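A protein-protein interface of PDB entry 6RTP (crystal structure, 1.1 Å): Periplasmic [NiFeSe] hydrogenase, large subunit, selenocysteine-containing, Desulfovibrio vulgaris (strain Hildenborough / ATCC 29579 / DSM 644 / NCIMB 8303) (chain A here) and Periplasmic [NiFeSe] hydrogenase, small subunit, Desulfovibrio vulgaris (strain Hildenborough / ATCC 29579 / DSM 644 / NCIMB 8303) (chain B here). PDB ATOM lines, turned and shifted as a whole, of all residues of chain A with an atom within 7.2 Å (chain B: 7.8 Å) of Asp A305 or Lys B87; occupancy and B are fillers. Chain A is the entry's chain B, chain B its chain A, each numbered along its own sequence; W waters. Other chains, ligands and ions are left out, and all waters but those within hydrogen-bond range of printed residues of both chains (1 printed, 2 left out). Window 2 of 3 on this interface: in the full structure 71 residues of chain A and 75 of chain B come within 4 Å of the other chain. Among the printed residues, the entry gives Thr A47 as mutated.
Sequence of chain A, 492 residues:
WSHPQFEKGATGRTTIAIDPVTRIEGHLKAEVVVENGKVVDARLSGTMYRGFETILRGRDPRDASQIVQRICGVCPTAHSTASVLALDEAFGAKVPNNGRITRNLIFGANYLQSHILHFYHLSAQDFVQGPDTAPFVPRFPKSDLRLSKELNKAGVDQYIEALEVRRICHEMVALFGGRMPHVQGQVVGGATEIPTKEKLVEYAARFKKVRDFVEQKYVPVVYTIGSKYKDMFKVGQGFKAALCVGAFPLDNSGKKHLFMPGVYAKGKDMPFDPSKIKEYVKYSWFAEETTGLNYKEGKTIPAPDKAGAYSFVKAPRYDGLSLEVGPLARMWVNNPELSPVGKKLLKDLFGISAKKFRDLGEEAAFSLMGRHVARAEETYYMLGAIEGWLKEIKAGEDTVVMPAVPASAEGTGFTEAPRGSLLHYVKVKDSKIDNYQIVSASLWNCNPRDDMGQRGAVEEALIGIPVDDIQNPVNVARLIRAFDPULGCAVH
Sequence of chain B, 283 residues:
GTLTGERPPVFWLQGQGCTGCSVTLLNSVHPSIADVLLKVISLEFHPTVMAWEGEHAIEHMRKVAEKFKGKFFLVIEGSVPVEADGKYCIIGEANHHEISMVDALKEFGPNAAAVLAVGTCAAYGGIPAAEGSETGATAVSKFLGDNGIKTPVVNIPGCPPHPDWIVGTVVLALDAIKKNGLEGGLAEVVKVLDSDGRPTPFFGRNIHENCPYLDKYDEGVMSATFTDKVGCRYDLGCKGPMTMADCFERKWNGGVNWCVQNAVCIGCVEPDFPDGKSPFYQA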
ATOM      1  N   GLY A  46      -7.781   3.027  11.110  1.00  0.00           N
ATOM      2  CA  GLY A  46      -8.470   3.869  12.065  1.00  0.00           C
ATOM      3  C   GLY A  46      -7.810   3.698  13.416  1.00  0.00           C
ATOM      4  O   GLY A  46      -7.817   2.599  13.978  1.00  0.00           O
ATOM      5  N   THR A  47      -7.205   4.766  13.926  1.00  0.00           N
ATOM      6  CA  THR A  47      -6.284   4.687  15.049  1.00  0.00           C
ATOM      7  C   THR A  47      -6.864   5.164  16.373  1.00  0.00           C
ATOM      8  O   THR A  47      -6.104   5.324  17.334  1.00  0.00           O
ATOM      9  CB  THR A  47      -5.027   5.493  14.714  1.00  0.00           C
ATOM     10  OG1 THR A  47      -5.416   6.786  14.258  1.00  0.00           O
ATOM     11  CG2 THR A  47      -4.219   4.821  13.630  1.00  0.00           C
ATOM     12  N   MET A  48      -8.181   5.353  16.476  1.00  0.00           N
ATOM     13  CA  MET A  48      -8.800   5.745  17.735  1.00  0.00           C
ATOM     14  C   MET A  48     -10.091   4.966  17.932  1.00  0.00           C
ATOM     15  O   MET A  48     -10.879   4.809  16.998  1.00  0.00           O
ATOM     16  CB  MET A  48      -9.071   7.252  17.781  1.00  0.00           C
ATOM     17  CG  MET A  48      -9.589   7.747  19.133  1.00  0.00           C
ATOM     18  SD  MET A  48     -11.392   7.628  19.362  1.00  0.00           S
ATOM     19  CE  MET A  48     -11.936   9.070  18.443  1.00  0.00           C
ATOM     20  N   TYR A  49     -10.298   4.490  19.154  1.00  0.00           N
ATOM     21  CA  TYR A  49     -11.473   3.702  19.514  1.00  0.00           C
ATOM     22  C   TYR A  49     -12.131   4.229  20.779  1.00  0.00           C
ATOM     23  O   TYR A  49     -11.447   4.585  21.742  1.00  0.00           O
ATOM     24  CB  TYR A  49     -11.068   2.225  19.711  1.00  0.00           C
ATOM     25  CG  TYR A  49     -12.157   1.307  20.205  1.00  0.00           C
ATOM     26  CD1 TYR A  49     -13.066   0.718  19.322  1.00  0.00           C
ATOM     27  CD2 TYR A  49     -12.255   0.980  21.556  1.00  0.00           C
ATOM     28  CE1 TYR A  49     -14.041  -0.144  19.772  1.00  0.00           C
ATOM     29  CE2 TYR A  49     -13.240   0.113  22.018  1.00  0.00           C
ATOM     30  CZ  TYR A  49     -14.126  -0.450  21.116  1.00  0.00           C
ATOM     31  OH  TYR A  49     -15.093  -1.325  21.557  1.00  0.00           O
ATOM     32  N   TRP A 285      -8.659  -4.743  15.126  1.00  0.00           N
ATOM     33  CA  TRP A 285      -8.283  -5.001  16.521  1.00  0.00           C
ATOM     34  C   TRP A 285      -9.499  -5.411  17.364  1.00  0.00           C
ATOM     35  O   TRP A 285      -9.902  -4.732  18.312  1.00  0.00           O
ATOM     36  CB  TRP A 285      -7.584  -3.779  17.102  1.00  0.00           C
ATOM     37  CG  TRP A 285      -6.203  -3.568  16.579  1.00  0.00           C
ATOM     38  CD1 TRP A 285      -5.182  -4.474  16.563  1.00  0.00           C
ATOM     39  CD2 TRP A 285      -5.688  -2.368  15.990  1.00  0.00           C
ATOM     40  NE1 TRP A 285      -4.068  -3.917  15.991  1.00  0.00           N
ATOM     41  CE2 TRP A 285      -4.350  -2.623  15.634  1.00  0.00           C
ATOM     42  CE3 TRP A 285      -6.225  -1.099  15.744  1.00  0.00           C
ATOM     43  CZ2 TRP A 285      -3.541  -1.662  15.030  1.00  0.00           C
ATOM     44  CZ3 TRP A 285      -5.414  -0.133  15.144  1.00  0.00           C
ATOM     45  CH2 TRP A 285      -4.091  -0.426  14.787  1.00  0.00           C
ATOM     46  N   PRO A 302     -12.813  -5.465  21.873  1.00  0.00           N
ATOM     47  CA  PRO A 302     -11.535  -4.943  21.382  1.00  0.00           C
ATOM     48  C   PRO A 302     -10.363  -5.863  21.703  1.00  0.00           C
ATOM     49  O   PRO A 302     -10.317  -6.536  22.738  1.00  0.00           O
ATOM     50  CB  PRO A 302     -11.415  -3.567  22.053  1.00  0.00           C
ATOM     51  CG  PRO A 302     -12.406  -3.544  23.131  1.00  0.00           C
ATOM     52  CD  PRO A 302     -13.464  -4.561  22.838  1.00  0.00           C
ATOM     53  N   ALA A 303      -9.403  -5.877  20.780  1.00  0.00           N
ATOM     54  CA  ALA A 303      -8.174  -6.657  20.914  1.00  0.00           C
ATOM     55  C   ALA A 303      -7.031  -5.836  20.341  1.00  0.00           C
ATOM     56  O   ALA A 303      -6.525  -6.117  19.249  1.00  0.00           O
ATOM     57  CB  ALA A 303      -8.314  -7.989  20.180  1.00  0.00           C
ATOM     58  N   PRO A 304      -6.592  -4.801  21.066  1.00  0.00           N
ATOM     59  CA  PRO A 304      -5.637  -3.839  20.492  1.00  0.00           C
ATOM     60  C   PRO A 304      -4.257  -4.399  20.263  1.00  0.00           C
ATOM     61  O   PRO A 304      -3.457  -3.738  19.589  1.00  0.00           O
ATOM     62  CB  PRO A 304      -5.594  -2.715  21.534  1.00  0.00           C
ATOM     63  CG  PRO A 304      -5.978  -3.365  22.802  1.00  0.00           C
ATOM     64  CD  PRO A 304      -7.012  -4.406  22.419  1.00  0.00           C
ATOM     65  N   ASP A 305      -3.941  -5.569  20.811  1.00  0.00           N
ATOM     66  CA  ASP A 305      -2.635  -6.187  20.625  1.00  0.00           C
ATOM     67  C   ASP A 305      -2.669  -7.352  19.645  1.00  0.00           C
ATOM     68  O   ASP A 305      -1.665  -8.060  19.507  1.00  0.00           O
ATOM     69  CB  ASP A 305      -2.073  -6.654  21.972  1.00  0.00           C
ATOM     70  CG  ASP A 305      -1.884  -5.510  22.952  1.00  0.00           C
ATOM     71  OD1 ASP A 305      -1.397  -4.444  22.525  1.00  0.00           O
ATOM     72  OD2 ASP A 305      -2.220  -5.670  24.143  1.00  0.00           O
ATOM     73  N   LYS A 306      -3.786  -7.579  18.964  1.00  0.00           N
ATOM     74  CA  LYS A 306      -3.882  -8.754  18.107  1.00  0.00           C
ATOM     75  C   LYS A 306      -2.932  -8.639  16.919  1.00  0.00           C
ATOM     76  O   LYS A 306      -2.954  -7.655  16.176  1.00  0.00           O
ATOM     77  CB  LYS A 306      -5.310  -8.965  17.620  1.00  0.00           C
ATOM     78  CG  LYS A 306      -5.469 -10.297  16.865  1.00  0.00           C
ATOM     79  CD  LYS A 306      -6.892 -10.510  16.375  1.00  0.00           C
ATOM     80  CE  LYS A 306      -7.219  -9.608  15.200  1.00  0.00           C
ATOM     81  NZ  LYS A 306      -8.606  -9.844  14.710  1.00  0.00           N
ATOM     82  N   ALA A 307      -2.107  -9.662  16.738  1.00  0.00           N
ATOM     83  CA  ALA A 307      -1.104  -9.652  15.687  1.00  0.00           C
ATOM     84  C   ALA A 307      -1.756  -9.578  14.314  1.00  0.00           C
ATOM     85  O   ALA A 307      -2.784 -10.206  14.066  1.00  0.00           O
ATOM     86  CB  ALA A 307      -0.293 -10.946  15.758  1.00  0.00           C
ATOM     87  N   GLY A 308      -1.136  -8.817  13.411  1.00  0.00           N
ATOM     88  CA  GLY A 308      -1.571  -8.744  12.036  1.00  0.00           C
ATOM     89  C   GLY A 308      -2.637  -7.706  11.757  1.00  0.00           C
ATOM     90  O   GLY A 308      -2.751  -7.247  10.613  1.00  0.00           O
ATOM     91  N   ALA A 309      -3.415  -7.316  12.764  1.00  0.00           N
ATOM     92  CA  ALA A 309      -4.466  -6.328  12.588  1.00  0.00           C
ATOM     93  C   ALA A 309      -3.852  -4.942  12.477  1.00  0.00           C
ATOM     94  O   ALA A 309      -2.755  -4.680  12.967  1.00  0.00           O
ATOM     95  CB  ALA A 309      -5.433  -6.374  13.769  1.00  0.00           C
ATOM     96  N   PHE A 312      -8.976  -0.114  13.949  1.00  0.00           N
ATOM     97  CA  PHE A 312     -10.163  -0.271  14.775  1.00  0.00           C
ATOM     98  C   PHE A 312     -11.456  -0.274  13.972  1.00  0.00           C
ATOM     99  O   PHE A 312     -12.524  -0.400  14.564  1.00  0.00           O
ATOM    100  CB  PHE A 312     -10.221   0.806  15.862  1.00  0.00           C
ATOM    101  CG  PHE A 312      -9.203   0.626  16.965  1.00  0.00           C
ATOM    102  CD1 PHE A 312      -9.273  -0.460  17.821  1.00  0.00           C
ATOM    103  CD2 PHE A 312      -8.209   1.564  17.173  1.00  0.00           C
ATOM    104  CE1 PHE A 312      -8.357  -0.609  18.855  1.00  0.00           C
ATOM    105  CE2 PHE A 312      -7.291   1.416  18.200  1.00  0.00           C
ATOM    106  CZ  PHE A 312      -7.371   0.321  19.042  1.00  0.00           C
ATOM    107  N   PRO B  81      -7.119   8.079  26.514  1.00  0.00           N
ATOM    108  CA  PRO B  81      -7.271   6.697  26.989  1.00  0.00           C
ATOM    109  C   PRO B  81      -5.930   6.113  27.382  1.00  0.00           C
ATOM    110  O   PRO B  81      -4.987   6.075  26.584  1.00  0.00           O
ATOM    111  CB  PRO B  81      -7.877   5.975  25.788  1.00  0.00           C
ATOM    112  CG  PRO B  81      -7.329   6.722  24.589  1.00  0.00           C
ATOM    113  CD  PRO B  81      -7.164   8.167  25.038  1.00  0.00           C
ATOM    114  N   VAL B  82      -5.851   5.595  28.606  1.00  0.00           N
ATOM    115  CA  VAL B  82      -4.585   5.099  29.132  1.00  0.00           C
ATOM    116  C   VAL B  82      -4.425   3.588  29.031  1.00  0.00           C
ATOM    117  O   VAL B  82      -3.302   3.099  29.203  1.00  0.00           O
ATOM    118  CB  VAL B  82      -4.355   5.565  30.584  1.00  0.00           C
ATOM    119  CG1 VAL B  82      -4.341   7.084  30.654  1.00  0.00           C
ATOM    120  CG2 VAL B  82      -5.376   4.961  31.540  1.00  0.00           C
ATOM    121  N   GLU B  83      -5.495   2.835  28.775  1.00  0.00           N
ATOM    122  CA  GLU B  83      -5.366   1.377  28.710  1.00  0.00           C
ATOM    123  C   GLU B  83      -4.542   0.953  27.498  1.00  0.00           C
ATOM    124  O   GLU B  83      -4.356   1.704  26.537  1.00  0.00           O
ATOM    125  CB  GLU B  83      -6.739   0.709  28.647  1.00  0.00           C
ATOM    126  CG  GLU B  83      -7.540   0.775  29.932  1.00  0.00           C
ATOM    127  CD  GLU B  83      -6.927  -0.004  31.064  1.00  0.00           C
ATOM    128  OE1 GLU B  83      -6.290  -1.032  30.790  1.00  0.00           O
ATOM    129  OE2 GLU B  83      -7.100   0.416  32.229  1.00  0.00           O
ATOM    130  N   ALA B  84      -4.023  -0.272  27.559  1.00  0.00           N
ATOM    131  CA  ALA B  84      -3.315  -0.855  26.425  1.00  0.00           C
ATOM    132  C   ALA B  84      -2.165   0.040  25.964  1.00  0.00           C
ATOM    133  O   ALA B  84      -1.927   0.222  24.770  1.00  0.00           O
ATOM    134  CB  ALA B  84      -4.275  -1.168  25.278  1.00  0.00           C
ATOM    135  N   ASP B  85      -1.456   0.623  26.927  1.00  0.00           N
ATOM    136  CA  ASP B  85      -0.283   1.446  26.642  1.00  0.00           C
ATOM    137  C   ASP B  85      -0.606   2.576  25.666  1.00  0.00           C
ATOM    138  O   ASP B  85       0.227   2.961  24.850  1.00  0.00           O
ATOM    139  CB  ASP B  85       0.879   0.595  26.128  1.00  0.00           C
ATOM    140  CG  ASP B  85       2.183   1.350  26.093  1.00  0.00           C
ATOM    141  OD1 ASP B  85       2.425   2.154  27.011  1.00  0.00           O
ATOM    142  OD2 ASP B  85       2.986   1.114  25.167  1.00  0.00           O
ATOM    143  N   GLY B  86      -1.819   3.110  25.732  1.00  0.00           N
ATOM    144  CA  GLY B  86      -2.200   4.264  24.937  1.00  0.00           C
ATOM    145  C   GLY B  86      -2.740   3.946  23.556  1.00  0.00           C
ATOM    146  O   GLY B  86      -3.096   4.873  22.822  1.00  0.00           O
ATOM    147  N   LYS B  87      -2.805   2.666  23.186  1.00  0.00           N
ATOM    148  CA  LYS B  87      -3.110   2.261  21.822  1.00  0.00           C
ATOM    149  C   LYS B  87      -4.519   2.599  21.377  1.00  0.00           C
ATOM    150  O   LYS B  87      -4.781   2.541  20.174  1.00  0.00           O
ATOM    151  CB  LYS B  87      -2.895   0.752  21.669  1.00  0.00           C
ATOM    152  CG  LYS B  87      -1.459   0.324  21.739  1.00  0.00           C
ATOM    153  CD  LYS B  87      -1.344  -1.155  21.369  1.00  0.00           C
ATOM    154  CE  LYS B  87       0.052  -1.699  21.556  1.00  0.00           C
ATOM    155  NZ  LYS B  87       0.167  -3.082  21.008  1.00  0.00           N
ATOM    156  N   TYR B  88      -5.429   2.933  22.285  1.00  0.00           N
ATOM    157  CA  TYR B  88      -6.776   3.290  21.846  1.00  0.00           C
ATOM    158  C   TYR B  88      -6.850   4.699  21.253  1.00  0.00           C
ATOM    159  O   TYR B  88      -7.914   5.100  20.778  1.00  0.00           O
ATOM    160  CB  TYR B  88      -7.793   3.099  22.973  1.00  0.00           C
ATOM    161  CG  TYR B  88      -8.044   1.654  23.344  1.00  0.00           C
ATOM    162  CD1 TYR B  88      -8.593   0.771  22.434  1.00  0.00           C
ATOM    163  CD2 TYR B  88      -7.786   1.188  24.627  1.00  0.00           C
ATOM    164  CE1 TYR B  88      -8.869  -0.526  22.773  1.00  0.00           C
ATOM    165  CE2 TYR B  88      -8.057  -0.116  24.975  1.00  0.00           C
ATOM    166  CZ  TYR B  88      -8.600  -0.968  24.043  1.00  0.00           C
ATOM    167  OH  TYR B  88      -8.888  -2.283  24.353  1.00  0.00           O
ATOM    168  N   CYS B  89      -5.746   5.452  21.220  1.00  0.00           N
ATOM    169  CA  CYS B  89      -5.732   6.721  20.492  1.00  0.00           C
ATOM    170  C   CYS B  89      -4.301   7.050  20.078  1.00  0.00           C
ATOM    171  O   CYS B  89      -3.499   7.493  20.904  1.00  0.00           O
ATOM    172  CB  CYS B  89      -6.320   7.859  21.309  1.00  0.00           C
ATOM    173  SG  CYS B  89      -6.446   9.370  20.353  1.00  0.00           S
ATOM    174  N   ILE B  90      -3.999   6.830  18.797  1.00  0.00           N
ATOM    175  CA  ILE B  90      -2.751   7.259  18.167  1.00  0.00           C
ATOM    176  C   ILE B  90      -3.075   8.491  17.333  1.00  0.00           C
ATOM    177  O   ILE B  90      -4.011   8.467  16.525  1.00  0.00           O
ATOM    178  CB  ILE B  90      -2.154   6.131  17.301  1.00  0.00           C
ATOM    179  CG1 ILE B  90      -1.838   4.882  18.137  1.00  0.00           C
ATOM    180  CG2 ILE B  90      -0.955   6.649  16.517  1.00  0.00           C
ATOM    181  CD1 ILE B  90      -0.975   5.133  19.299  1.00  0.00           C
ATOM    182  N   GLU B  98       5.068   5.841  16.380  1.00  0.00           N
ATOM    183  CA  GLU B  98       3.700   6.258  16.650  1.00  0.00           C
ATOM    184  C   GLU B  98       3.673   7.159  17.875  1.00  0.00           C
ATOM    185  O   GLU B  98       4.479   7.012  18.799  1.00  0.00           O
ATOM    186  CB  GLU B  98       2.817   5.044  16.935  1.00  0.00           C
ATOM    187  CG  GLU B  98       2.683   4.066  15.806  1.00  0.00           C
ATOM    188  CD  GLU B  98       2.025   2.777  16.248  1.00  0.00           C
ATOM    189  OE1 GLU B  98       1.577   2.702  17.415  1.00  0.00           O
ATOM    190  OE2 GLU B  98       1.963   1.842  15.426  1.00  0.00           O
ATOM    191  N   SER B 100       1.010   8.267  20.695  1.00  0.00           N
ATOM    192  CA  SER B 100      -0.303   8.120  21.298  1.00  0.00           C
ATOM    193  C   SER B 100      -0.746   9.448  21.902  1.00  0.00           C
ATOM    194  O   SER B 100       0.041  10.386  22.068  1.00  0.00           O
ATOM    195  CB  SER B 100      -0.289   7.046  22.376  1.00  0.00           C
ATOM    196  OG  SER B 100       0.473   7.499  23.490  1.00  0.00           O
ATOM    197  N   MET B 101      -2.035   9.538  22.235  1.00  0.00           N
ATOM    198  CA  MET B 101      -2.508  10.725  22.934  1.00  0.00           C
ATOM    199  C   MET B 101      -1.818  10.869  24.283  1.00  0.00           C
ATOM    200  O   MET B 101      -1.473  11.982  24.691  1.00  0.00           O
ATOM    201  CB  MET B 101      -4.028  10.711  23.097  1.00  0.00           C
ATOM    202  CG  MET B 101      -4.569  11.987  23.705  1.00  0.00           C
ATOM    203  SD  MET B 101      -4.363  13.358  22.557  1.00  0.00           S
ATOM    204  CE  MET B 101      -5.398  14.559  23.343  1.00  0.00           C
ATOM    205  N   VAL B 102      -1.589   9.757  24.973  1.00  0.00           N
ATOM    206  CA  VAL B 102      -0.788   9.769  26.199  1.00  0.00           C
ATOM    207  C   VAL B 102       0.568  10.409  25.938  1.00  0.00           C
ATOM    208  O   VAL B 102       0.997  11.305  26.665  1.00  0.00           O
ATOM    209  CB  VAL B 102      -0.645   8.335  26.739  1.00  0.00           C
ATOM    210  CG1 VAL B 102       0.488   8.223  27.755  1.00  0.00           C
ATOM    211  CG2 VAL B 102      -1.955   7.861  27.338  1.00  0.00           C
ATOM    212  N   THR B 135     -11.539   1.676  27.704  1.00  0.00           N
ATOM    213  CA  THR B 135     -10.292   2.217  27.175  1.00  0.00           C
ATOM    214  C   THR B 135      -9.471   2.995  28.199  1.00  0.00           C
ATOM    215  O   THR B 135      -8.403   3.511  27.855  1.00  0.00           O
ATOM    216  CB  THR B 135     -10.548   3.117  25.957  1.00  0.00           C
ATOM    217  OG1 THR B 135     -11.294   4.269  26.356  1.00  0.00           O
ATOM    218  CG2 THR B 135     -11.267   2.350  24.844  1.00  0.00           C
HETATM  219  O   HOH W   1      -1.028  -3.554  18.341  1.00  0.00           O
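Printed residues of chain A that touch a printed residue of chain B: Thr A47, Met A48, Tyr A49, Pro A302, Pro A304, Asp A305 and Phe A312. Hydrophobic or aromatic side chains of chain A within 4 Å of the printed part of chain B: Met A48, Tyr A49, Pro A302, Pro A304 and Phe A312. Of the 15 printed residues of chain B, 6 touch a printed residue of chain A. Hydrophobic or aromatic side chains of chain B within 4 Å of the printed part of chain A: Ala B84, Tyr B88 and Ile B90. Among the printed residues, 14 pairs touch across the chains. Among the printed residues, Asp or Glu carboxylates within 4 Å of a Lys or Arg side-chain nitrogen of the other chain: Asp A305 with Lys B87 (2.6 Å).
N of Phe A312 lies within hydrogen-bond range of O of Gly A46, 3.0 Å away. O of Cys B89 lies within hydrogen-bond range of N of Met B101. O of Thr B135 is in hydrogen-bond range of N of Glu B83 (3.1 Å). The backbone NH (N) of Val B82 is in hydrogen-bond range of the backbone carbonyl oxygen (O) of Thr B135 (3.4 Å).
Asp A305 touches just one residue of chain B: Lys B87 (2.6 Å). Of chain A, only Pro A304 (3.8 Å), Asp A305 (2.6 Å) and Phe A312 (3.4 Å) come within 4 Å of Lys B87. Pro A304 touches just these residues of chain B: Ala B84 (3.7 Å), Lys B87 (3.8 Å) and Tyr B88 (3.4 Å). No residue of chain A comes within 4 Å of Gly B86. Of the printed residues of chain A, Tyr B88 touches Thr A47, Met A48, Tyr A49, Pro A302, Pro A304 and Phe A312. Of the printed residues of chain B, Tyr A49 touches Tyr B88 and Thr B135. Printed residues of chain A within 4 Å of Ile B90: Thr A47 (3.0 Å). Ser B100 touches none of the printed residues of chain A. Met B101 touches none of the printed residues of chain A.
The backbone NH (N) of Tyr A49 sits at hydrogen-bond distance from the backbone carbonyl oxygen (O) of Tyr B88 (2.9 Å). The backbone carbonyl oxygen (O) of Thr A47 lies within hydrogen-bond range of the backbone NH (N) of Ile B90, at 3.0 Å. OD1 of Asp A305 lies within salt-bridge range of NZ of Lys B87, 2.6 Å away.
Water W1 lies within hydrogen-bond range of the backbone carbonyl oxygen (O) of Pro A304 (2.7 Å) and the side-chain amino group (NZ) of Lys B87 (3.0 Å).
Among the printed residues, merely in contact across the chains: Met A48 with Tyr B88 (3.2 Å), Phe A312 with Lys B87 (3.4 Å), Pro A304 with Tyr B88 (3.4 Å), Thr A47 with Cys B89 (3.5 Å), Phe A312 with Tyr B88 (3.6 Å), Pro A302 with Tyr B88 (3.7 Å), Tyr A49 with Thr B135 (3.7 Å), Pro A304 with Ala B84 (3.7 Å), Met A48 with Cys B89 (3.7 Å), Pro A304 with Lys B87 (3.8 Å) and Thr A47 with Tyr B88 (3.9 Å).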
